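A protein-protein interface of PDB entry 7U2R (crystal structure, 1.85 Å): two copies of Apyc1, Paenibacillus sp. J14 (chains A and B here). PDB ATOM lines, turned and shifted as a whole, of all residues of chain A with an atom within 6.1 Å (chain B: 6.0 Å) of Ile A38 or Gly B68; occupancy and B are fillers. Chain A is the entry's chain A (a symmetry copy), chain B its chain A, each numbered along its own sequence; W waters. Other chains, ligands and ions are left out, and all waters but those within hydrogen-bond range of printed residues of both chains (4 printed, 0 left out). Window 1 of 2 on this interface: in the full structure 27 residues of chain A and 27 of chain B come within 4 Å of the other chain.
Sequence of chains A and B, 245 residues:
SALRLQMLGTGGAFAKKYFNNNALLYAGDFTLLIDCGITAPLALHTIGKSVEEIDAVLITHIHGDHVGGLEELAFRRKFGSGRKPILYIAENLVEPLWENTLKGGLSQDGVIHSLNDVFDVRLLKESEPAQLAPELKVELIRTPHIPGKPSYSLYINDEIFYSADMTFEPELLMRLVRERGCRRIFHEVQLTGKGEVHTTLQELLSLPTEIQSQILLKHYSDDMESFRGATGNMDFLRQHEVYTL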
ATOM      1  N   ALA A  13       6.464  -1.614  11.038  1.00  0.00           N
ATOM      2  CA  ALA A  13       5.247  -2.419  10.889  1.00  0.00           C
ATOM      3  C   ALA A  13       4.417  -2.483  12.165  1.00  0.00           C
ATOM      4  O   ALA A  13       3.184  -2.566  12.098  1.00  0.00           O
ATOM      5  CB  ALA A  13       5.613  -3.854  10.457  1.00  0.00           C
ATOM      6  N   ASN A  20       1.435   3.204   9.542  1.00  0.00           N
ATOM      7  CA  ASN A  20       2.299   2.436   8.638  1.00  0.00           C
ATOM      8  C   ASN A  20       3.017   3.392   7.677  1.00  0.00           C
ATOM      9  O   ASN A  20       2.495   4.452   7.316  1.00  0.00           O
ATOM     10  CB  ASN A  20       1.502   1.449   7.755  1.00  0.00           C
ATOM     11  CG  ASN A  20       0.783   0.349   8.505  1.00  0.00           C
ATOM     12  OD1 ASN A  20      -0.135  -0.247   7.933  1.00  0.00           O
ATOM     13  ND2 ASN A  20       1.183   0.035   9.737  1.00  0.00           N
ATOM     14  N   ASN A  22       3.695   4.884   4.718  1.00  0.00           N
ATOM     15  CA  ASN A  22       3.055   5.014   3.422  1.00  0.00           C
ATOM     16  C   ASN A  22       3.117   6.490   3.058  1.00  0.00           C
ATOM     17  O   ASN A  22       2.907   7.343   3.915  1.00  0.00           O
ATOM     18  CB  ASN A  22       1.542   4.574   3.416  1.00  0.00           C
ATOM     19  CG  ASN A  22       1.267   3.176   4.003  1.00  0.00           C
ATOM     20  OD1 ASN A  22       0.150   2.947   4.475  1.00  0.00           O
ATOM     21  ND2 ASN A  22       2.224   2.237   3.926  1.00  0.00           N
ATOM     22  N   CYS A  36       0.069   1.124   1.014  1.00  0.00           N
ATOM     23  CA  CYS A  36      -1.297   1.291   1.494  1.00  0.00           C
ATOM     24  C   CYS A  36      -1.524   0.206   2.533  1.00  0.00           C
ATOM     25  O   CYS A  36      -2.120  -0.829   2.220  1.00  0.00           O
ATOM     26  CB  CYS A  36      -2.289   1.164   0.318  1.00  0.00           C
ATOM     27  SG  CYS A  36      -4.006   1.538   0.793  1.00  0.00           S
ATOM     28  N   GLY A  37      -0.952   0.405   3.730  1.00  0.00           N
ATOM     29  CA  GLY A  37      -1.004  -0.562   4.811  1.00  0.00           C
ATOM     30  C   GLY A  37      -2.328  -0.610   5.553  1.00  0.00           C
ATOM     31  O   GLY A  37      -3.302   0.082   5.235  1.00  0.00           O
ATOM     32  N   ILE A  38      -2.370  -1.510   6.543  1.00  0.00           N
ATOM     33  CA  ILE A  38      -3.577  -1.687   7.342  1.00  0.00           C
ATOM     34  C   ILE A  38      -4.002  -0.365   8.001  1.00  0.00           C
ATOM     35  O   ILE A  38      -5.182  -0.188   8.294  1.00  0.00           O
ATOM     36  CB  ILE A  38      -3.386  -2.805   8.397  1.00  0.00           C
ATOM     37  CG1 ILE A  38      -2.266  -2.446   9.392  1.00  0.00           C
ATOM     38  CG2 ILE A  38      -3.177  -4.174   7.723  1.00  0.00           C
ATOM     39  CD1 ILE A  38      -2.086  -3.483  10.569  1.00  0.00           C
ATOM     40  N   THR A  39      -3.061   0.575   8.258  1.00  0.00           N
ATOM     41  CA  THR A  39      -3.458   1.872   8.827  1.00  0.00           C
ATOM     42  C   THR A  39      -3.744   2.950   7.794  1.00  0.00           C
ATOM     43  O   THR A  39      -4.147   4.062   8.195  1.00  0.00           O
ATOM     44  CB  THR A  39      -2.382   2.465   9.748  1.00  0.00           C
ATOM     45  OG1 THR A  39      -1.187   2.650   8.970  1.00  0.00           O
ATOM     46  CG2 THR A  39      -2.072   1.535  10.946  1.00  0.00           C
ATOM     47  N   ALA A  40      -3.518   2.697   6.497  1.00  0.00           N
ATOM     48  CA  ALA A  40      -3.655   3.789   5.539  1.00  0.00           C
ATOM     49  C   ALA A  40      -5.081   4.354   5.526  1.00  0.00           C
ATOM     50  O   ALA A  40      -5.225   5.586   5.493  1.00  0.00           O
ATOM     51  CB  ALA A  40      -3.220   3.325   4.132  1.00  0.00           C
ATOM     52  N   PRO A  41      -6.156   3.557   5.574  1.00  0.00           N
ATOM     53  CA  PRO A  41      -7.489   4.198   5.645  1.00  0.00           C
ATOM     54  C   PRO A  41      -7.654   5.137   6.837  1.00  0.00           C
ATOM     55  O   PRO A  41      -8.212   6.250   6.699  1.00  0.00           O
ATOM     56  CB  PRO A  41      -8.449   3.000   5.722  1.00  0.00           C
ATOM     57  CG  PRO A  41      -7.664   1.837   4.980  1.00  0.00           C
ATOM     58  CD  PRO A  41      -6.234   2.071   5.431  1.00  0.00           C
ATOM     59  N   LEU A  42      -7.233   4.704   8.026  1.00  0.00           N
ATOM     60  CA  LEU A  42      -7.365   5.591   9.177  1.00  0.00           C
ATOM     61  C   LEU A  42      -6.467   6.816   9.023  1.00  0.00           C
ATOM     62  O   LEU A  42      -6.850   7.937   9.400  1.00  0.00           O
ATOM     63  CB  LEU A  42      -7.034   4.828  10.462  1.00  0.00           C
ATOM     64  CG  LEU A  42      -7.253   5.553  11.793  1.00  0.00           C
ATOM     65  CD1 LEU A  42      -8.680   6.189  11.905  1.00  0.00           C
ATOM     66  CD2 LEU A  42      -7.070   4.500  12.895  1.00  0.00           C
ATOM     67  N   GLY A  64       1.752  -6.619   5.201  1.00  0.00           N
ATOM     68  CA  GLY A  64       0.520  -5.987   5.618  1.00  0.00           C
ATOM     69  C   GLY A  64       0.643  -4.492   5.813  1.00  0.00           C
ATOM     70  O   GLY A  64      -0.327  -3.751   5.581  1.00  0.00           O
ATOM     71  N   ASP A  65       1.819  -4.013   6.250  1.00  0.00           N
ATOM     72  CA  ASP A  65       1.919  -2.571   6.455  1.00  0.00           C
ATOM     73  C   ASP A  65       2.118  -1.812   5.150  1.00  0.00           C
ATOM     74  O   ASP A  65       2.255  -0.577   5.177  1.00  0.00           O
ATOM     75  CB  ASP A  65       3.039  -2.228   7.473  1.00  0.00           C
ATOM     76  CG  ASP A  65       4.378  -2.882   7.151  1.00  0.00           C
ATOM     77  OD1 ASP A  65       4.419  -4.085   6.778  1.00  0.00           O
ATOM     78  OD2 ASP A  65       5.385  -2.188   7.357  1.00  0.00           O
ATOM     79  N   HIS A  66       2.103  -2.523   4.008  1.00  0.00           N
ATOM     80  CA  HIS A  66       2.162  -1.904   2.692  1.00  0.00           C
ATOM     81  C   HIS A  66       1.028  -2.295   1.761  1.00  0.00           C
ATOM     82  O   HIS A  66       0.815  -1.580   0.776  1.00  0.00           O
ATOM     83  CB  HIS A  66       3.513  -2.253   2.004  1.00  0.00           C
ATOM     84  CG  HIS A  66       4.669  -1.854   2.849  1.00  0.00           C
ATOM     85  ND1 HIS A  66       5.325  -0.654   2.685  1.00  0.00           N
ATOM     86  CD2 HIS A  66       5.182  -2.411   3.972  1.00  0.00           C
ATOM     87  CE1 HIS A  66       6.254  -0.531   3.612  1.00  0.00           C
ATOM     88  NE2 HIS A  66       6.185  -1.583   4.402  1.00  0.00           N
ATOM     89  N   VAL A  67       0.275  -3.368   2.029  1.00  0.00           N
ATOM     90  CA  VAL A  67      -0.828  -3.677   1.110  1.00  0.00           C
ATOM     91  C   VAL A  67      -2.141  -3.929   1.849  1.00  0.00           C
ATOM     92  O   VAL A  67      -3.188  -4.125   1.219  1.00  0.00           O
ATOM     93  CB  VAL A  67      -0.500  -4.881   0.207  1.00  0.00           C
ATOM     94  CG1 VAL A  67       0.724  -4.599  -0.688  1.00  0.00           C
ATOM     95  CG2 VAL A  67      -0.281  -6.157   1.051  1.00  0.00           C
ATOM     96  N   GLY A  68      -2.091  -3.959   3.179  1.00  0.00           N
ATOM     97  CA  GLY A  68      -3.228  -4.398   3.954  1.00  0.00           C
ATOM     98  C   GLY A  68      -4.421  -3.465   3.941  1.00  0.00           C
ATOM     99  O   GLY A  68      -5.488  -3.864   4.419  1.00  0.00           O
ATOM    100  N   GLY A  69      -4.266  -2.231   3.443  1.00  0.00           N
ATOM    101  CA  GLY A  69      -5.368  -1.304   3.302  1.00  0.00           C
ATOM    102  C   GLY A  69      -5.976  -1.279   1.903  1.00  0.00           C
ATOM    103  O   GLY A  69      -6.943  -0.545   1.671  1.00  0.00           O
ATOM    104  N   CYS B  36     -10.161 -10.157  13.670  1.00  0.00           N
ATOM    105  CA  CYS B  36      -8.887  -9.478  13.869  1.00  0.00           C
ATOM    106  C   CYS B  36      -8.630  -8.665  12.611  1.00  0.00           C
ATOM    107  O   CYS B  36      -7.873  -9.104  11.740  1.00  0.00           O
ATOM    108  CB  CYS B  36      -7.768 -10.513  14.111  1.00  0.00           C
ATOM    109  SG  CYS B  36      -6.175  -9.749  14.549  1.00  0.00           S
ATOM    110  N   GLY B  37      -9.347  -7.539  12.478  1.00  0.00           N
ATOM    111  CA  GLY B  37      -9.283  -6.683  11.308  1.00  0.00           C
ATOM    112  C   GLY B  37      -8.049  -5.800  11.237  1.00  0.00           C
ATOM    113  O   GLY B  37      -7.147  -5.836  12.081  1.00  0.00           O
ATOM    114  N   ILE B  38      -7.994  -5.020  10.150  1.00  0.00           N
ATOM    115  CA  ILE B  38      -6.866  -4.124   9.928  1.00  0.00           C
ATOM    116  C   ILE B  38      -6.691  -3.155  11.109  1.00  0.00           C
ATOM    117  O   ILE B  38      -5.582  -2.679  11.341  1.00  0.00           O
ATOM    118  CB  ILE B  38      -7.018  -3.358   8.592  1.00  0.00           C
ATOM    119  CG1 ILE B  38      -8.275  -2.467   8.601  1.00  0.00           C
ATOM    120  CG2 ILE B  38      -6.974  -4.323   7.391  1.00  0.00           C
ATOM    121  CD1 ILE B  38      -8.441  -1.564   7.316  1.00  0.00           C
ATOM    122  N   THR B  39      -7.769  -2.836  11.865  1.00  0.00           N
ATOM    123  CA  THR B  39      -7.609  -1.964  13.037  1.00  0.00           C
ATOM    124  C   THR B  39      -7.361  -2.704  14.343  1.00  0.00           C
ATOM    125  O   THR B  39      -7.152  -2.032  15.374  1.00  0.00           O
ATOM    126  CB  THR B  39      -8.846  -1.090  13.295  1.00  0.00           C
ATOM    127  OG1 THR B  39      -9.966  -1.963  13.521  1.00  0.00           O
ATOM    128  CG2 THR B  39      -9.155  -0.161  12.095  1.00  0.00           C
ATOM    129  N   PRO B  41      -4.828  -4.414  15.677  1.00  0.00           N
ATOM    130  CA  PRO B  41      -3.607  -4.036  16.423  1.00  0.00           C
ATOM    131  C   PRO B  41      -3.692  -2.664  17.088  1.00  0.00           C
ATOM    132  O   PRO B  41      -3.276  -2.494  18.256  1.00  0.00           O
ATOM    133  CB  PRO B  41      -2.510  -4.082  15.346  1.00  0.00           C
ATOM    134  CG  PRO B  41      -3.053  -5.147  14.300  1.00  0.00           C
ATOM    135  CD  PRO B  41      -4.540  -4.848  14.276  1.00  0.00           C
ATOM    136  N   HIS B  63     -12.655 -11.159   5.242  1.00  0.00           N
ATOM    137  CA  HIS B  63     -12.783  -9.776   4.818  1.00  0.00           C
ATOM    138  C   HIS B  63     -11.750  -9.015   5.624  1.00  0.00           C
ATOM    139  O   HIS B  63     -11.452  -9.396   6.760  1.00  0.00           O
ATOM    140  CB  HIS B  63     -14.144  -9.175   5.149  1.00  0.00           C
ATOM    141  CG  HIS B  63     -15.116  -9.170   4.029  1.00  0.00           C
ATOM    142  ND1 HIS B  63     -16.463  -9.088   4.268  1.00  0.00           N
ATOM    143  CD2 HIS B  63     -14.967  -9.190   2.683  1.00  0.00           C
ATOM    144  CE1 HIS B  63     -17.116  -9.128   3.113  1.00  0.00           C
ATOM    145  NE2 HIS B  63     -16.228  -9.146   2.135  1.00  0.00           N
ATOM    146  N   GLY B  64     -11.242  -7.922   5.058  1.00  0.00           N
ATOM    147  CA  GLY B  64     -10.155  -7.224   5.708  1.00  0.00           C
ATOM    148  C   GLY B  64     -10.494  -6.743   7.102  1.00  0.00           C
ATOM    149  O   GLY B  64      -9.611  -6.686   7.974  1.00  0.00           O
ATOM    150  N   ASP B  65     -11.763  -6.374   7.344  1.00  0.00           N
ATOM    151  CA  ASP B  65     -12.074  -5.890   8.686  1.00  0.00           C
ATOM    152  C   ASP B  65     -12.231  -7.026   9.690  1.00  0.00           C
ATOM    153  O   ASP B  65     -12.532  -6.762  10.867  1.00  0.00           O
ATOM    154  CB  ASP B  65     -13.330  -4.981   8.675  1.00  0.00           C
ATOM    155  CG  ASP B  65     -14.529  -5.604   7.970  1.00  0.00           C
ATOM    156  OD1 ASP B  65     -14.372  -6.221   6.883  1.00  0.00           O
ATOM    157  OD2 ASP B  65     -15.636  -5.393   8.491  1.00  0.00           O
ATOM    158  N   HIS B  66     -12.003  -8.276   9.255  1.00  0.00           N
ATOM    159  CA  HIS B  66     -12.002  -9.433  10.141  1.00  0.00           C
ATOM    160  C   HIS B  66     -10.733 -10.266  10.087  1.00  0.00           C
ATOM    161  O   HIS B  66     -10.515 -11.046  11.022  1.00  0.00           O
ATOM    162  CB  HIS B  66     -13.215 -10.350   9.812  1.00  0.00           C
ATOM    163  CG  HIS B  66     -14.497  -9.600   9.889  1.00  0.00           C
ATOM    164  ND1 HIS B  66     -15.283  -9.598  11.020  1.00  0.00           N
ATOM    165  CD2 HIS B  66     -15.047  -8.695   9.046  1.00  0.00           C
ATOM    166  CE1 HIS B  66     -16.313  -8.796  10.835  1.00  0.00           C
ATOM    167  NE2 HIS B  66     -16.191  -8.238   9.648  1.00  0.00           N
ATOM    168  N   VAL B  67      -9.879 -10.130   9.067  1.00  0.00           N
ATOM    169  CA  VAL B  67      -8.654 -10.939   9.089  1.00  0.00           C
ATOM    170  C   VAL B  67      -7.406 -10.102   8.819  1.00  0.00           C
ATOM    171  O   VAL B  67      -6.281 -10.616   8.880  1.00  0.00           O
ATOM    172  CB  VAL B  67      -8.723 -12.107   8.086  1.00  0.00           C
ATOM    173  CG1 VAL B  67      -9.872 -13.078   8.428  1.00  0.00           C
ATOM    174  CG2 VAL B  67      -8.860 -11.581   6.640  1.00  0.00           C
ATOM    175  N   GLY B  68      -7.590  -8.825   8.489  1.00  0.00           N
ATOM    176  CA  GLY B  68      -6.495  -8.015   8.014  1.00  0.00           C
ATOM    177  C   GLY B  68      -5.441  -7.678   9.047  1.00  0.00           C
ATOM    178  O   GLY B  68      -4.387  -7.155   8.668  1.00  0.00           O
ATOM    179  N   GLY B  69      -5.704  -7.925  10.337  1.00  0.00           N
ATOM    180  CA  GLY B  69      -4.724  -7.726  11.384  1.00  0.00           C
ATOM    181  C   GLY B  69      -3.980  -8.996  11.782  1.00  0.00           C
ATOM    182  O   GLY B  69      -3.099  -8.942  12.648  1.00  0.00           O
ATOM    183  N   LEU B  70      -4.316 -10.138  11.165  1.00  0.00           N
ATOM    184  CA  LEU B  70      -3.714 -11.415  11.575  1.00  0.00           C
ATOM    185  C   LEU B  70      -2.230 -11.477  11.240  1.00  0.00           C
ATOM    186  O   LEU B  70      -1.468 -12.122  11.965  1.00  0.00           O
ATOM    187  CB  LEU B  70      -4.432 -12.593  10.908  1.00  0.00           C
ATOM    188  CG  LEU B  70      -5.809 -12.905  11.480  1.00  0.00           C
ATOM    189  CD1 LEU B  70      -6.466 -14.017  10.648  1.00  0.00           C
ATOM    190  CD2 LEU B  70      -5.722 -13.319  12.949  1.00  0.00           C
ATOM    191  N   GLU B  71      -1.802 -10.853  10.139  1.00  0.00           N
ATOM    192  CA  GLU B  71      -0.381 -10.877   9.810  1.00  0.00           C
ATOM    193  C   GLU B  71       0.435 -10.218  10.915  1.00  0.00           C
ATOM    194  O   GLU B  71       1.461 -10.769  11.352  1.00  0.00           O
ATOM    195  CB  GLU B  71      -0.110 -10.205   8.463  1.00  0.00           C
ATOM    196  CG  GLU B  71       1.386 -10.091   8.166  1.00  0.00           C
ATOM    197  CD  GLU B  71       1.700  -9.415   6.840  1.00  0.00           C
ATOM    198  OE1 GLU B  71       1.127  -9.808   5.811  1.00  0.00           O
ATOM    199  OE2 GLU B  71       2.522  -8.473   6.821  1.00  0.00           O
ATOM    200  N   GLU B  72      -0.017  -9.039  11.386  1.00  0.00           N
ATOM    201  CA  GLU B  72       0.700  -8.354  12.468  1.00  0.00           C
ATOM    202  C   GLU B  72       0.663  -9.169  13.760  1.00  0.00           C
ATOM    203  O   GLU B  72       1.691  -9.311  14.437  1.00  0.00           O
ATOM    204  CB  GLU B  72       0.128  -6.947  12.697  1.00  0.00           C
ATOM    205  CG  GLU B  72       0.698  -6.311  13.970  1.00  0.00           C
ATOM    206  CD  GLU B  72       0.591  -4.783  14.052  1.00  0.00           C
ATOM    207  OE1 GLU B  72       0.143  -4.160  13.059  1.00  0.00           O
ATOM    208  OE2 GLU B  72       0.961  -4.213  15.124  1.00  0.00           O
ATOM    209  N   THR B 101      -5.065 -14.981   1.331  1.00  0.00           N
ATOM    210  CA  THR B 101      -5.102 -13.810   2.216  1.00  0.00           C
ATOM    211  C   THR B 101      -3.788 -13.612   2.976  1.00  0.00           C
ATOM    212  O   THR B 101      -3.175 -12.538   2.881  1.00  0.00           O
ATOM    213  CB  THR B 101      -6.268 -13.899   3.205  1.00  0.00           C
ATOM    214  OG1 THR B 101      -7.498 -13.917   2.492  1.00  0.00           O
ATOM    215  CG2 THR B 101      -6.294 -12.680   4.152  1.00  0.00           C
HETATM  216  O   HOH W   1       1.141  -3.692  10.572  1.00  0.00           O
HETATM  217  O   HOH W   2       4.074  -6.581   8.426  1.00  0.00           O
HETATM  218  O   HOH W   3       0.038  -8.914   3.443  1.00  0.00           O
HETATM  219  O   HOH W   4       0.822  -1.223  12.828  1.00  0.00           O
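The side-chain carboxylate (OE2) of Glu B71 lies within hydrogen-bond range of the backbone NH (N) of Gly A64, 2.6 Å away.
Water W1 bridges the side-chain carboxylate of Glu B72 (2.7 Å) and the backbone carbonyl oxygen of Ala A13 (2.8 Å).
Water W3 lies within hydrogen-bond range of OE1 of Glu B71 (2.8 Å) and N of Gly A64 (3.4 Å).
Water W4 lies within hydrogen-bond range of O of Ala A13, OE1 of Glu B72 and ND2 of Asn A20.
Water W2 lies within hydrogen-bond range of the side-chain carboxylate (OE2) of Glu B71 (2.9 Å) and the side-chain carboxylate (OD1) of Asp A65 (3.0 Å).
Among the printed residues, merely in contact across the chains: Ile A38 with Gly B68, Gly A68 with Ile B38, Ile A38 with Glu B72, Ala A13 with Glu B72 and Ile A38 with Ile B38.
Of the printed residues of chain B, Ala A13 touches Glu B72 (3.6 Å).
Printed residues of chain B within 4 Å of Ile A38: Ile B38 (3.7 Å), Gly B68 (3.4 Å) and Glu B72 (3.4 Å).
Of the printed residues of chain B, Gly A64 touches Glu B71.
Printed residues of chain B within 4 Å of Gly A68: Ile B38 (3.4 Å).
Gly B37 touches none of the printed residues of chain A.
Of the printed residues of chain A, Ile B38 touches Ile A38 (3.7 Å) and Gly A68 (3.4 Å).
Asp B65 touches none of the printed residues of chain A.
Of the printed residues of chain A, Gly B68 touches Ile A38 (3.4 Å).
Printed residues of chain A within 4 Å of Glu B71: Gly A64 (2.6 Å).
The backbone carbonyl oxygen of Cys A36 is in hydrogen-bond range of the backbone NH of Gly A68, at 3.3 Å.
N of Ile B38 lies within hydrogen-bond range of O of Gly B64.
N of Ile A38 lies within hydrogen-bond range of OD1 of Asn A20 (2.9 Å).
The backbone NH (N) of Gly B68 lies within hydrogen-bond range of the backbone carbonyl oxygen (O) of Cys B36 (3.3 Å).
The backbone carbonyl oxygen of Gly A64 sits at hydrogen-bond distance from the backbone NH of Ile A38.
Ile B38 touches its own counterpart, Ile A38.
Ile A38 touches Gly B68, and with the chains exchanged Gly A68 touches Ile B38.
Of the 16 printed residues of chain B, 4 touch a printed residue of chain A.
Printed residues of chain B that touch a printed residue of chain A: Ile B38, Gly B68, Glu B71 and Glu B72.
Hydrophobic or aromatic side chains of chain B within 4 Å of the printed part of chain A: Ile B38.
Of the 16 printed residues of chain A, 4 touch a printed residue of chain B.
Printed residues of chain A that touch a printed residue of chain B: Ala A13, Ile A38, Gly A64 and Gly A68.
Among the printed residues, no Asp or Glu carboxylate lies within 4 Å of a Lys or Arg side-chain nitrogen of the other chain.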
